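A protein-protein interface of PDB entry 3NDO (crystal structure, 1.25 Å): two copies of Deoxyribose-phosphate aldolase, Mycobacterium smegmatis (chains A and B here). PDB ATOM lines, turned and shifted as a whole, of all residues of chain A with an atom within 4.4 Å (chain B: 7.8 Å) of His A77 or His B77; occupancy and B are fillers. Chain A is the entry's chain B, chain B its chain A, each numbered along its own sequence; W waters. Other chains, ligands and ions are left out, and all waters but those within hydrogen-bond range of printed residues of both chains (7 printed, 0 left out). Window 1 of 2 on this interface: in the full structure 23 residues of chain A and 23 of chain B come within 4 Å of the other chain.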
ATOM      1  N   PRO A  51     -15.045  17.155   2.436  1.00  0.00           N
ATOM      2  CA  PRO A  51     -16.084  17.637   3.300  1.00  0.00           C
ATOM      3  C   PRO A  51     -15.688  18.878   4.059  1.00  0.00           C
ATOM      4  O   PRO A  51     -16.534  19.438   4.741  1.00  0.00           O
ATOM      5  CB  PRO A  51     -16.309  16.483   4.239  1.00  0.00           C
ATOM      6  CG  PRO A  51     -15.690  15.327   3.679  1.00  0.00           C
ATOM      7  CD  PRO A  51     -14.583  15.811   2.860  1.00  0.00           C
ATOM      8  N   GLY A  71     -10.777  11.270  -4.939  1.00  0.00           N
ATOM      9  CA  GLY A  71     -10.412   9.872  -5.013  1.00  0.00           C
ATOM     10  C   GLY A  71      -9.328   9.481  -4.040  1.00  0.00           C
ATOM     11  O   GLY A  71      -8.577   8.558  -4.356  1.00  0.00           O
ATOM     12  N   PHE A  72      -9.234  10.168  -2.932  1.00  0.00           N
ATOM     13  CA  PHE A  72      -8.014  10.184  -2.111  1.00  0.00           C
ATOM     14  C   PHE A  72      -8.219   9.497  -0.783  1.00  0.00           C
ATOM     15  O   PHE A  72      -9.248   9.675  -0.136  1.00  0.00           O
ATOM     16  CB  PHE A  72      -7.632  11.664  -1.906  1.00  0.00           C
ATOM     17  CG  PHE A  72      -6.371  11.897  -1.140  1.00  0.00           C
ATOM     18  CD1 PHE A  72      -5.213  12.288  -1.801  1.00  0.00           C
ATOM     19  CD2 PHE A  72      -6.331  11.814   0.261  1.00  0.00           C
ATOM     20  CE1 PHE A  72      -4.042  12.498  -1.088  1.00  0.00           C
ATOM     21  CE2 PHE A  72      -5.165  12.050   0.963  1.00  0.00           C
ATOM     22  CZ  PHE A  72      -4.020  12.386   0.275  1.00  0.00           C
ATOM     23  N   SER A  74      -6.721   6.472  -1.801  1.00  0.00           N
ATOM     24  CA  SER A  74      -6.468   5.167  -2.411  1.00  0.00           C
ATOM     25  C   SER A  74      -6.445   5.193  -3.920  1.00  0.00           C
ATOM     26  O   SER A  74      -5.864   4.274  -4.491  1.00  0.00           O
ATOM     27  CB  SER A  74      -7.481   4.158  -1.954  1.00  0.00           C
ATOM     28  OG  SER A  74      -8.726   4.345  -2.533  1.00  0.00           O
ATOM     29  N   GLY A  75      -7.158   6.092  -4.571  1.00  0.00           N
ATOM     30  CA  GLY A  75      -7.386   6.019  -5.987  1.00  0.00           C
ATOM     31  C   GLY A  75      -8.406   4.975  -6.413  1.00  0.00           C
ATOM     32  O   GLY A  75      -8.680   4.866  -7.599  1.00  0.00           O
ATOM     33  N   LYS A  76      -8.943   4.205  -5.475  1.00  0.00           N
ATOM     34  CA  LYS A  76      -9.827   3.063  -5.775  1.00  0.00           C
ATOM     35  C   LYS A  76     -11.269   3.482  -5.708  1.00  0.00           C
ATOM     36  O   LYS A  76     -12.036   3.131  -4.820  1.00  0.00           O
ATOM     37  CB  LYS A  76      -9.510   1.863  -4.876  1.00  0.00           C
ATOM     38  CG  LYS A  76      -8.232   1.148  -5.284  1.00  0.00           C
ATOM     39  CD  LYS A  76      -8.351   0.515  -6.647  1.00  0.00           C
ATOM     40  CE  LYS A  76      -7.272  -0.561  -6.822  1.00  0.00           C
ATOM     41  NZ  LYS A  76      -7.112  -0.859  -8.190  1.00  0.00           N
ATOM     42  N   HIS A  77     -11.632   4.267  -6.719  1.00  0.00           N
ATOM     43  CA  HIS A  77     -12.994   4.804  -6.866  1.00  0.00           C
ATOM     44  C   HIS A  77     -13.248   4.767  -8.347  1.00  0.00           C
ATOM     45  O   HIS A  77     -12.315   5.016  -9.116  1.00  0.00           O
ATOM     46  CB  HIS A  77     -13.127   6.230  -6.337  1.00  0.00           C
ATOM     47  CG  HIS A  77     -12.691   6.371  -4.918  1.00  0.00           C
ATOM     48  ND1 HIS A  77     -13.480   6.116  -3.819  1.00  0.00           N
ATOM     49  CD2 HIS A  77     -11.462   6.711  -4.422  1.00  0.00           C
ATOM     50  CE1 HIS A  77     -12.756   6.276  -2.723  1.00  0.00           C
ATOM     51  NE2 HIS A  77     -11.538   6.671  -3.052  1.00  0.00           N
ATOM     52  N   VAL A  78     -14.462   4.520  -8.782  1.00  0.00           N
ATOM     53  CA  VAL A  78     -14.718   4.532 -10.198  1.00  0.00           C
ATOM     54  C   VAL A  78     -14.618   5.967 -10.752  1.00  0.00           C
ATOM     55  O   VAL A  78     -14.791   6.936 -10.023  1.00  0.00           O
ATOM     56  CB  VAL A  78     -16.053   3.837 -10.558  1.00  0.00           C
ATOM     57  CG1 VAL A  78     -16.031   2.400 -10.103  1.00  0.00           C
ATOM     58  CG2 VAL A  78     -17.270   4.661 -10.056  1.00  0.00           C
ATOM     59  N   PRO A  79     -14.369   6.111 -12.065  1.00  0.00           N
ATOM     60  CA  PRO A  79     -14.178   7.483 -12.611  1.00  0.00           C
ATOM     61  C   PRO A  79     -15.284   8.469 -12.306  1.00  0.00           C
ATOM     62  O   PRO A  79     -15.064   9.631 -12.045  1.00  0.00           O
ATOM     63  CB  PRO A  79     -14.067   7.256 -14.111  1.00  0.00           C
ATOM     64  CG  PRO A  79     -13.496   5.878 -14.225  1.00  0.00           C
ATOM     65  CD  PRO A  79     -14.059   5.111 -13.085  1.00  0.00           C
ATOM     66  N   ILE A  81     -17.266   8.618  -9.833  1.00  0.00           N
ATOM     67  CA  ILE A  81     -17.216   9.050  -8.430  1.00  0.00           C
ATOM     68  C   ILE A  81     -16.104  10.092  -8.256  1.00  0.00           C
ATOM     69  O   ILE A  81     -16.313  11.102  -7.604  1.00  0.00           O
ATOM     70  CB  ILE A  81     -17.048   7.836  -7.510  1.00  0.00           C
ATOM     71  CG1 ILE A  81     -18.376   7.064  -7.441  1.00  0.00           C
ATOM     72  CG2 ILE A  81     -16.563   8.290  -6.121  1.00  0.00           C
ATOM     73  CD1 ILE A  81     -19.484   7.767  -6.728  1.00  0.00           C
ATOM     74  N   LYS A  82     -14.913   9.846  -8.797  1.00  0.00           N
ATOM     75  CA  LYS A  82     -13.882  10.858  -8.730  1.00  0.00           C
ATOM     76  C   LYS A  82     -14.306  12.159  -9.338  1.00  0.00           C
ATOM     77  O   LYS A  82     -14.031  13.234  -8.805  1.00  0.00           O
ATOM     78  CB  LYS A  82     -12.568  10.374  -9.389  1.00  0.00           C
ATOM     79  CG  LYS A  82     -11.978   9.158  -8.715  1.00  0.00           C
ATOM     80  CD  LYS A  82     -10.595   8.791  -9.317  1.00  0.00           C
ATOM     81  CE  LYS A  82     -10.035   7.548  -8.751  1.00  0.00           C
ATOM     82  NZ  LYS A  82      -8.829   7.066  -9.409  1.00  0.00           N
ATOM     83  N   GLU A  85     -16.939  13.863  -7.151  1.00  0.00           N
ATOM     84  CA  GLU A  85     -16.285  14.411  -5.976  1.00  0.00           C
ATOM     85  C   GLU A  85     -15.570  15.717  -6.291  1.00  0.00           C
ATOM     86  O   GLU A  85     -15.674  16.680  -5.532  1.00  0.00           O
ATOM     87  CB  GLU A  85     -15.347  13.385  -5.388  1.00  0.00           C
ATOM     88  CG  GLU A  85     -14.584  13.856  -4.211  1.00  0.00           C
ATOM     89  CD  GLU A  85     -14.198  12.675  -3.319  1.00  0.00           C
ATOM     90  OE1 GLU A  85     -13.134  12.037  -3.584  1.00  0.00           O
ATOM     91  OE2 GLU A  85     -14.954  12.313  -2.353  1.00  0.00           O
ATOM     92  N   SER B  49     -12.259  -3.342  -3.360  1.00  0.00           N
ATOM     93  CA  SER B  49     -12.499  -1.944  -3.626  1.00  0.00           C
ATOM     94  C   SER B  49     -13.554  -1.780  -4.714  1.00  0.00           C
ATOM     95  O   SER B  49     -13.724  -2.631  -5.579  1.00  0.00           O
ATOM     96  CB  SER B  49     -11.226  -1.232  -4.093  1.00  0.00           C
ATOM     97  OG  SER B  49     -10.190  -1.310  -3.110  1.00  0.00           O
ATOM     98  N   PRO B  50     -14.242  -0.630  -4.739  1.00  0.00           N
ATOM     99  CA  PRO B  50     -15.322  -0.446  -5.708  1.00  0.00           C
ATOM    100  C   PRO B  50     -15.037  -0.708  -7.170  1.00  0.00           C
ATOM    101  O   PRO B  50     -15.895  -1.348  -7.816  1.00  0.00           O
ATOM    102  CB  PRO B  50     -15.748   1.018  -5.472  1.00  0.00           C
ATOM    103  CG  PRO B  50     -15.408   1.266  -4.036  1.00  0.00           C
ATOM    104  CD  PRO B  50     -14.244   0.440  -3.715  1.00  0.00           C
ATOM    105  N   PRO B  51     -13.898  -0.297  -7.704  1.00  0.00           N
ATOM    106  CA  PRO B  51     -13.657  -0.554  -9.129  1.00  0.00           C
ATOM    107  C   PRO B  51     -13.347  -1.999  -9.434  1.00  0.00           C
ATOM    108  O   PRO B  51     -13.221  -2.313 -10.604  1.00  0.00           O
ATOM    109  CB  PRO B  51     -12.427   0.347  -9.474  1.00  0.00           C
ATOM    110  CG  PRO B  51     -12.182   1.101  -8.291  1.00  0.00           C
ATOM    111  CD  PRO B  51     -12.841   0.575  -7.131  1.00  0.00           C
ATOM    112  N   LEU B  52     -13.175  -2.846  -8.428  1.00  0.00           N
ATOM    113  CA  LEU B  52     -12.823  -4.241  -8.595  1.00  0.00           C
ATOM    114  C   LEU B  52     -13.967  -5.191  -8.286  1.00  0.00           C
ATOM    115  O   LEU B  52     -13.815  -6.408  -8.416  1.00  0.00           O
ATOM    116  CB  LEU B  52     -11.546  -4.555  -7.804  1.00  0.00           C
ATOM    117  CG  LEU B  52     -10.292  -3.960  -8.453  1.00  0.00           C
ATOM    118  CD1 LEU B  52      -9.165  -3.829  -7.431  1.00  0.00           C
ATOM    119  CD2 LEU B  52      -9.854  -4.801  -9.630  1.00  0.00           C
ATOM    120  N   VAL B  69     -16.080  -1.777  -0.131  1.00  0.00           N
ATOM    121  CA  VAL B  69     -15.921  -0.639   0.769  1.00  0.00           C
ATOM    122  C   VAL B  69     -16.478   0.634   0.116  1.00  0.00           C
ATOM    123  O   VAL B  69     -16.508   0.766  -1.078  1.00  0.00           O
ATOM    124  CB  VAL B  69     -14.441  -0.480   1.203  1.00  0.00           C
ATOM    125  CG1 VAL B  69     -13.983  -1.636   2.044  1.00  0.00           C
ATOM    126  CG2 VAL B  69     -13.502  -0.262   0.016  1.00  0.00           C
ATOM    127  N   ALA B  70     -16.900   1.582   0.923  1.00  0.00           N
ATOM    128  CA  ALA B  70     -17.381   2.867   0.472  1.00  0.00           C
ATOM    129  C   ALA B  70     -16.835   3.978   1.337  1.00  0.00           C
ATOM    130  O   ALA B  70     -16.764   3.855   2.561  1.00  0.00           O
ATOM    131  CB  ALA B  70     -18.935   2.925   0.488  1.00  0.00           C
ATOM    132  N   GLY B  71     -16.442   5.069   0.724  1.00  0.00           N
ATOM    133  CA  GLY B  71     -15.827   6.139   1.434  1.00  0.00           C
ATOM    134  C   GLY B  71     -14.506   5.787   2.067  1.00  0.00           C
ATOM    135  O   GLY B  71     -14.155   6.374   3.088  1.00  0.00           O
ATOM    136  N   PHE B  72     -13.751   4.853   1.462  1.00  0.00           N
ATOM    137  CA  PHE B  72     -12.687   4.143   2.153  1.00  0.00           C
ATOM    138  C   PHE B  72     -11.325   4.479   1.563  1.00  0.00           C
ATOM    139  O   PHE B  72     -11.189   4.579   0.338  1.00  0.00           O
ATOM    140  CB  PHE B  72     -12.999   2.655   1.976  1.00  0.00           C
ATOM    141  CG  PHE B  72     -12.034   1.701   2.651  1.00  0.00           C
ATOM    142  CD1 PHE B  72     -12.369   1.087   3.837  1.00  0.00           C
ATOM    143  CD2 PHE B  72     -10.785   1.414   2.084  1.00  0.00           C
ATOM    144  CE1 PHE B  72     -11.487   0.223   4.466  1.00  0.00           C
ATOM    145  CE2 PHE B  72      -9.922   0.560   2.742  1.00  0.00           C
ATOM    146  CZ  PHE B  72     -10.290  -0.033   3.929  1.00  0.00           C
ATOM    147  N   PRO B  73     -10.280   4.609   2.386  1.00  0.00           N
ATOM    148  CA  PRO B  73     -10.277   4.382   3.836  1.00  0.00           C
ATOM    149  C   PRO B  73     -10.496   5.599   4.682  1.00  0.00           C
ATOM    150  O   PRO B  73     -10.609   5.450   5.911  1.00  0.00           O
ATOM    151  CB  PRO B  73      -8.844   3.868   4.095  1.00  0.00           C
ATOM    152  CG  PRO B  73      -8.050   4.622   3.085  1.00  0.00           C
ATOM    153  CD  PRO B  73      -8.911   4.673   1.838  1.00  0.00           C
ATOM    154  N   SER B  74     -10.525   6.806   4.126  1.00  0.00           N
ATOM    155  CA  SER B  74     -10.458   8.003   4.936  1.00  0.00           C
ATOM    156  C   SER B  74     -11.730   8.397   5.605  1.00  0.00           C
ATOM    157  O   SER B  74     -11.670   9.107   6.619  1.00  0.00           O
ATOM    158  CB  SER B  74      -9.917   9.180   4.169  1.00  0.00           C
ATOM    159  OG  SER B  74     -10.946   9.682   3.270  1.00  0.00           O
ATOM    160  N   GLY B  75     -12.883   8.025   5.044  1.00  0.00           N
ATOM    161  CA  GLY B  75     -14.145   8.539   5.491  1.00  0.00           C
ATOM    162  C   GLY B  75     -14.403   9.962   5.068  1.00  0.00           C
ATOM    163  O   GLY B  75     -15.479  10.508   5.369  1.00  0.00           O
ATOM    164  N   LYS B  76     -13.455  10.611   4.419  1.00  0.00           N
ATOM    165  CA  LYS B  76     -13.557  12.073   4.120  1.00  0.00           C
ATOM    166  C   LYS B  76     -14.132  12.263   2.717  1.00  0.00           C
ATOM    167  O   LYS B  76     -13.438  12.652   1.775  1.00  0.00           O
ATOM    168  CB  LYS B  76     -12.213  12.762   4.288  1.00  0.00           C
ATOM    169  CG  LYS B  76     -11.804  12.980   5.723  1.00  0.00           C
ATOM    170  CD  LYS B  76     -12.767  13.925   6.449  1.00  0.00           C
ATOM    171  CE  LYS B  76     -12.101  14.487   7.696  1.00  0.00           C
ATOM    172  NZ  LYS B  76     -13.069  15.022   8.601  1.00  0.00           N
ATOM    173  N   HIS B  77     -15.405  11.952   2.595  1.00  0.00           N
ATOM    174  CA  HIS B  77     -16.173  12.097   1.372  1.00  0.00           C
ATOM    175  C   HIS B  77     -17.530  12.583   1.788  1.00  0.00           C
ATOM    176  O   HIS B  77     -18.005  12.199   2.841  1.00  0.00           O
ATOM    177  CB  HIS B  77     -16.292  10.768   0.634  1.00  0.00           C
ATOM    178  CG  HIS B  77     -14.990  10.067   0.384  1.00  0.00           C
ATOM    179  ND1 HIS B  77     -14.208  10.342  -0.711  1.00  0.00           N
ATOM    180  CD2 HIS B  77     -14.295   9.205   1.156  1.00  0.00           C
ATOM    181  CE1 HIS B  77     -13.093   9.619  -0.608  1.00  0.00           C
ATOM    182  NE2 HIS B  77     -13.136   8.903   0.504  1.00  0.00           N
ATOM    183  N   VAL B  78     -18.172  13.419   1.000  1.00  0.00           N
ATOM    184  CA  VAL B  78     -19.486  13.918   1.396  1.00  0.00           C
ATOM    185  C   VAL B  78     -20.520  12.775   1.263  1.00  0.00           C
ATOM    186  O   VAL B  78     -20.312  11.806   0.529  1.00  0.00           O
ATOM    187  CB  VAL B  78     -19.883  15.176   0.578  1.00  0.00           C
ATOM    188  CG1 VAL B  78     -18.847  16.269   0.796  1.00  0.00           C
ATOM    189  CG2 VAL B  78     -20.110  14.888  -0.882  1.00  0.00           C
ATOM    190  N   PRO B  79     -21.671  12.885   1.948  1.00  0.00           N
ATOM    191  CA  PRO B  79     -22.634  11.790   1.957  1.00  0.00           C
ATOM    192  C   PRO B  79     -23.099  11.361   0.606  1.00  0.00           C
ATOM    193  O   PRO B  79     -23.297  10.182   0.342  1.00  0.00           O
ATOM    194  CB  PRO B  79     -23.766  12.314   2.858  1.00  0.00           C
ATOM    195  CG  PRO B  79     -23.118  13.201   3.776  1.00  0.00           C
ATOM    196  CD  PRO B  79     -22.021  13.884   2.976  1.00  0.00           C
ATOM    197  N   GLY B  80     -23.353  12.315  -0.289  1.00  0.00           N
ATOM    198  CA  GLY B  80     -23.834  12.015  -1.625  1.00  0.00           C
ATOM    199  C   GLY B  80     -22.836  11.133  -2.383  1.00  0.00           C
ATOM    200  O   GLY B  80     -23.236  10.228  -3.147  1.00  0.00           O
ATOM    201  N   ILE B  81     -21.550  11.316  -2.150  1.00  0.00           N
ATOM    202  CA  ILE B  81     -20.513  10.496  -2.808  1.00  0.00           C
ATOM    203  C   ILE B  81     -20.464   9.124  -2.182  1.00  0.00           C
ATOM    204  O   ILE B  81     -20.426   8.138  -2.915  1.00  0.00           O
ATOM    205  CB  ILE B  81     -19.124  11.202  -2.667  1.00  0.00           C
ATOM    206  CG1 ILE B  81     -19.081  12.424  -3.552  1.00  0.00           C
ATOM    207  CG2 ILE B  81     -17.984  10.237  -2.959  1.00  0.00           C
ATOM    208  CD1 ILE B  81     -19.144  12.148  -5.094  1.00  0.00           C
ATOM    209  N   LYS B  82     -20.492   9.001  -0.857  1.00  0.00           N
ATOM    210  CA  LYS B  82     -20.495   7.689  -0.252  1.00  0.00           C
ATOM    211  C   LYS B  82     -21.689   6.869  -0.731  1.00  0.00           C
ATOM    212  O   LYS B  82     -21.585   5.673  -0.984  1.00  0.00           O
ATOM    213  CB  LYS B  82     -20.477   7.749   1.266  1.00  0.00           C
ATOM    214  CG  LYS B  82     -19.221   8.360   1.838  1.00  0.00           C
ATOM    215  CD  LYS B  82     -19.135   8.291   3.386  1.00  0.00           C
ATOM    216  CE  LYS B  82     -17.981   9.001   3.924  1.00  0.00           C
ATOM    217  NZ  LYS B  82     -17.994   9.101   5.402  1.00  0.00           N
ATOM    218  N   ALA B  83     -22.856   7.485  -0.742  1.00  0.00           N
ATOM    219  CA  ALA B  83     -24.072   6.798  -1.121  1.00  0.00           C
ATOM    220  C   ALA B  83     -24.035   6.358  -2.564  1.00  0.00           C
ATOM    221  O   ALA B  83     -24.408   5.242  -2.877  1.00  0.00           O
ATOM    222  CB  ALA B  83     -25.276   7.698  -0.836  1.00  0.00           C
ATOM    223  N   GLU B  85     -21.361   5.875  -4.418  1.00  0.00           N
ATOM    224  CA  GLU B  85     -20.357   4.820  -4.527  1.00  0.00           C
ATOM    225  C   GLU B  85     -20.910   3.484  -4.115  1.00  0.00           C
ATOM    226  O   GLU B  85     -20.679   2.476  -4.785  1.00  0.00           O
ATOM    227  CB  GLU B  85     -19.147   5.224  -3.682  1.00  0.00           C
ATOM    228  CG  GLU B  85     -18.073   4.166  -3.637  1.00  0.00           C
ATOM    229  CD  GLU B  85     -16.745   4.772  -3.347  1.00  0.00           C
ATOM    230  OE1 GLU B  85     -16.386   4.951  -2.169  1.00  0.00           O
ATOM    231  OE2 GLU B  85     -15.949   5.067  -4.251  1.00  0.00           O
ATOM    232  N   VAL B 100     -17.066   3.876   5.649  1.00  0.00           N
ATOM    233  CA  VAL B 100     -16.318   4.508   6.681  1.00  0.00           C
ATOM    234  C   VAL B 100     -16.999   5.796   7.116  1.00  0.00           C
ATOM    235  O   VAL B 100     -17.406   6.575   6.256  1.00  0.00           O
ATOM    236  CB  VAL B 100     -14.862   4.844   6.246  1.00  0.00           C
ATOM    237  CG1 VAL B 100     -14.080   5.351   7.434  1.00  0.00           C
ATOM    238  CG2 VAL B 100     -14.237   3.628   5.616  1.00  0.00           C
ATOM    239  N   ILE B 101     -17.160   6.026   8.416  1.00  0.00           N
ATOM    240  CA  ILE B 101     -17.668   7.298   8.894  1.00  0.00           C
ATOM    241  C   ILE B 101     -16.656   8.398   8.684  1.00  0.00           C
ATOM    242  O   ILE B 101     -15.467   8.166   8.469  1.00  0.00           O
ATOM    243  CB  ILE B 101     -18.046   7.201  10.439  1.00  0.00           C
ATOM    244  CG1 ILE B 101     -16.811   7.087  11.307  1.00  0.00           C
ATOM    245  CG2 ILE B 101     -19.078   6.157  10.734  1.00  0.00           C
ATOM    246  CD1 ILE B 101     -17.008   7.397  12.781  1.00  0.00           C
ATOM    247  N   ASP B 102     -17.122   9.638   8.800  1.00  0.00           N
ATOM    248  CA  ASP B 102     -16.269  10.781   8.957  1.00  0.00           C
ATOM    249  C   ASP B 102     -15.843  10.871  10.417  1.00  0.00           C
ATOM    250  O   ASP B 102     -16.579  11.313  11.297  1.00  0.00           O
ATOM    251  CB  ASP B 102     -16.990  12.033   8.442  1.00  0.00           C
ATOM    252  CG  ASP B 102     -16.102  13.283   8.459  1.00  0.00           C
ATOM    253  OD1 ASP B 102     -15.127  13.329   9.248  1.00  0.00           O
ATOM    254  OD2 ASP B 102     -16.415  14.212   7.674  1.00  0.00           O
ATOM    255  N   ASP B 117     -24.824  10.877   7.223  1.00  0.00           N
ATOM    256  CA  ASP B 117     -23.976  10.153   6.314  1.00  0.00           C
ATOM    257  C   ASP B 117     -24.369   8.677   6.208  1.00  0.00           C
ATOM    258  O   ASP B 117     -24.591   8.115   5.113  1.00  0.00           O
ATOM    259  CB  ASP B 117     -22.551  10.324   6.822  1.00  0.00           C
ATOM    260  CG  ASP B 117     -21.501   9.844   5.959  1.00  0.00           C
ATOM    261  OD1 ASP B 117     -21.597   9.987   4.720  1.00  0.00           O
ATOM    262  OD2 ASP B 117     -20.452   9.291   6.511  1.00  0.00           O
HETATM  263  O   HOH W   1      -9.603   6.536  -1.123  1.00  0.00           O
HETATM  264  O   HOH W   2     -16.290   4.088  -6.694  1.00  0.00           O
HETATM  265  O   HOH W   3     -15.611   8.101  -2.726  1.00  0.00           O
HETATM  266  O   HOH W   4     -10.824   7.722   1.336  1.00  0.00           O
HETATM  267  O   HOH W   5     -11.824   2.964  -2.039  1.00  0.00           O
HETATM  268  O   HOH W   6     -10.903  11.980   0.799  1.00  0.00           O
HETATM  269  O   HOH W   7     -16.739  14.023  -1.329  1.00  0.00           O
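Pro A51 touches Lys B76, and with the chains exchanged Lys A76 touches Pro B51. Phe A72 touches Ser B74, and with the chains exchanged Ser A74 touches Phe B72. Phe A72 touches His B77, and with the chains exchanged His A77 touches Phe B72. His B77 touches its own counterpart, His A77. Positions printed for both chains: 51, 71, 72, 74, 75, 76, 77, 78, 79, 81, 82 and 85. Of the 19 pairs that touch across the chains among the printed residues, 16 have their exchanged pair printed and touching as well.
Printed residues of chain B that touch a printed residue of chain A: Ser B49, Pro B50, Pro B51, Leu B52, Phe B72, Ser B74, Lys B76, His B77, Val B78, Ile B81 and Glu B85. Hydrophobic or aromatic side chains of chain B that line the printed part of chain A: Pro B50, Pro B51, Leu B52, His B77, Val B78 and Ile B81. Of the 12 printed residues of chain A, 8 touch a printed residue of chain B. Printed residues of chain A that touch a printed residue of chain B: Pro A51, Phe A72, Ser A74, Lys A76, His A77, Val A78, Ile A81 and Glu A85.
Water W2 bridges OE2 of Glu B85 (2.7 Å) and N of Val A78 (2.8 Å). Water W7 lies within hydrogen-bond range of the side-chain carboxylate (OE2) of Glu A85 (2.7 Å) and the backbone NH (N) of Val B78 (2.8 Å). Water W4 lies within hydrogen-bond range of a ring nitrogen (NE2) of His B77 (2.7 Å), the side-chain hydroxyl (OG) of Ser B74 (2.8 Å), the backbone carbonyl oxygen (O) of Phe A72 (2.9 Å) and the backbone carbonyl oxygen (O) of Phe B72 (3.3 Å). Water W5 lies within hydrogen-bond range of O of Lys A76 (2.8 Å), O of Phe B72 (2.9 Å) and OG of Ser A74 (3.4 Å). Water W6 lies within hydrogen-bond range of O of Lys B76, O of Phe A72 and OG of Ser B74. Water W3 lies within hydrogen-bond range of ND1 of His A77, OE1 of Glu B85 and ND1 of His B77.
ND1 of His B77 lies within hydrogen-bond range of OE2 of Glu A85. A ring nitrogen (ND1) of His A77 is in hydrogen-bond range of the side-chain carboxylate (OE2) of Glu B85 (2.7 Å).
Printed residues of chain B within 4 Å of Phe A72: Ser B74 and His B77. Of chain B, only Pro B51 (3.6 Å), Phe B72 (3.8 Å), His B77 (3.97 Å) and Glu B85 (2.7 Å) come within 4 Å of His A77. Of the printed residues of chain A, Pro B50 touches Lys A76 (3.7 Å). Ala B70 touches none of the printed residues of chain A. Gly B75 touches none of the printed residues of chain A. His B77 touches just these residues of chain A: Pro A51, Phe A72, His A77 and Glu A85. Of the printed residues of chain A, Ile B81 touches Ile A81 (3.9 Å) and Glu A85 (3.5 Å). Printed residues of chain A within 4 Å of Glu B85: His A77 (2.7 Å) and Ile A81 (3.5 Å). The nearest printed residue of chain A that does not touch His B77 is Gly A71 (5.1 Å). The nearest printed residue of chain A that does not touch Pro B50 is Val A78 (4.4 Å).
Among the printed residues, merely in contact across the chains: Glu A85 with Ile B81 (3.5 Å), Ile A81 with Glu B85 (3.5 Å), Pro A51 with Lys B76 (3.5 Å), Lys A76 with Pro B51 (3.5 Å), Pro A51 with His B77 (3.6 Å), His A77 with Pro B51 (3.6 Å), Lys A76 with Ser B49 (3.6 Å), Lys A76 with Pro B50 (3.7 Å), Lys A76 with Leu B52 (3.7 Å), Ser A74 with Phe B72 (3.8 Å), Phe A72 with Ser B74 (3.8 Å), His A77 with Phe B72 (3.8 Å), Phe A72 with His B77 (3.9 Å), Val A78 with Pro B51 (3.9 Å), Ile A81 with Ile B81 (3.9 Å), His A77 with His B77 (3.97 Å) and Pro A51 with Val B78 (3.97 Å).
N of Gly B71 is in hydrogen-bond range of OE1 of Glu B85 (2.9 Å). The side-chain hydroxyl (OG) of Ser B74 lies within hydrogen-bond range of the backbone NH (N) of Lys B76, 2.9 Å away. The side-chain carboxylate (OD1) of Asp B102 lies within salt-bridge range of the side-chain amino group (NZ) of Lys B76 (2.7 Å). The side-chain carboxylate (OE1) of Glu A85 sits at hydrogen-bond distance from the backbone NH (N) of Gly A71 (2.8 Å). N of Lys A76 is in hydrogen-bond range of OG of Ser A74, 3.0 Å away.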
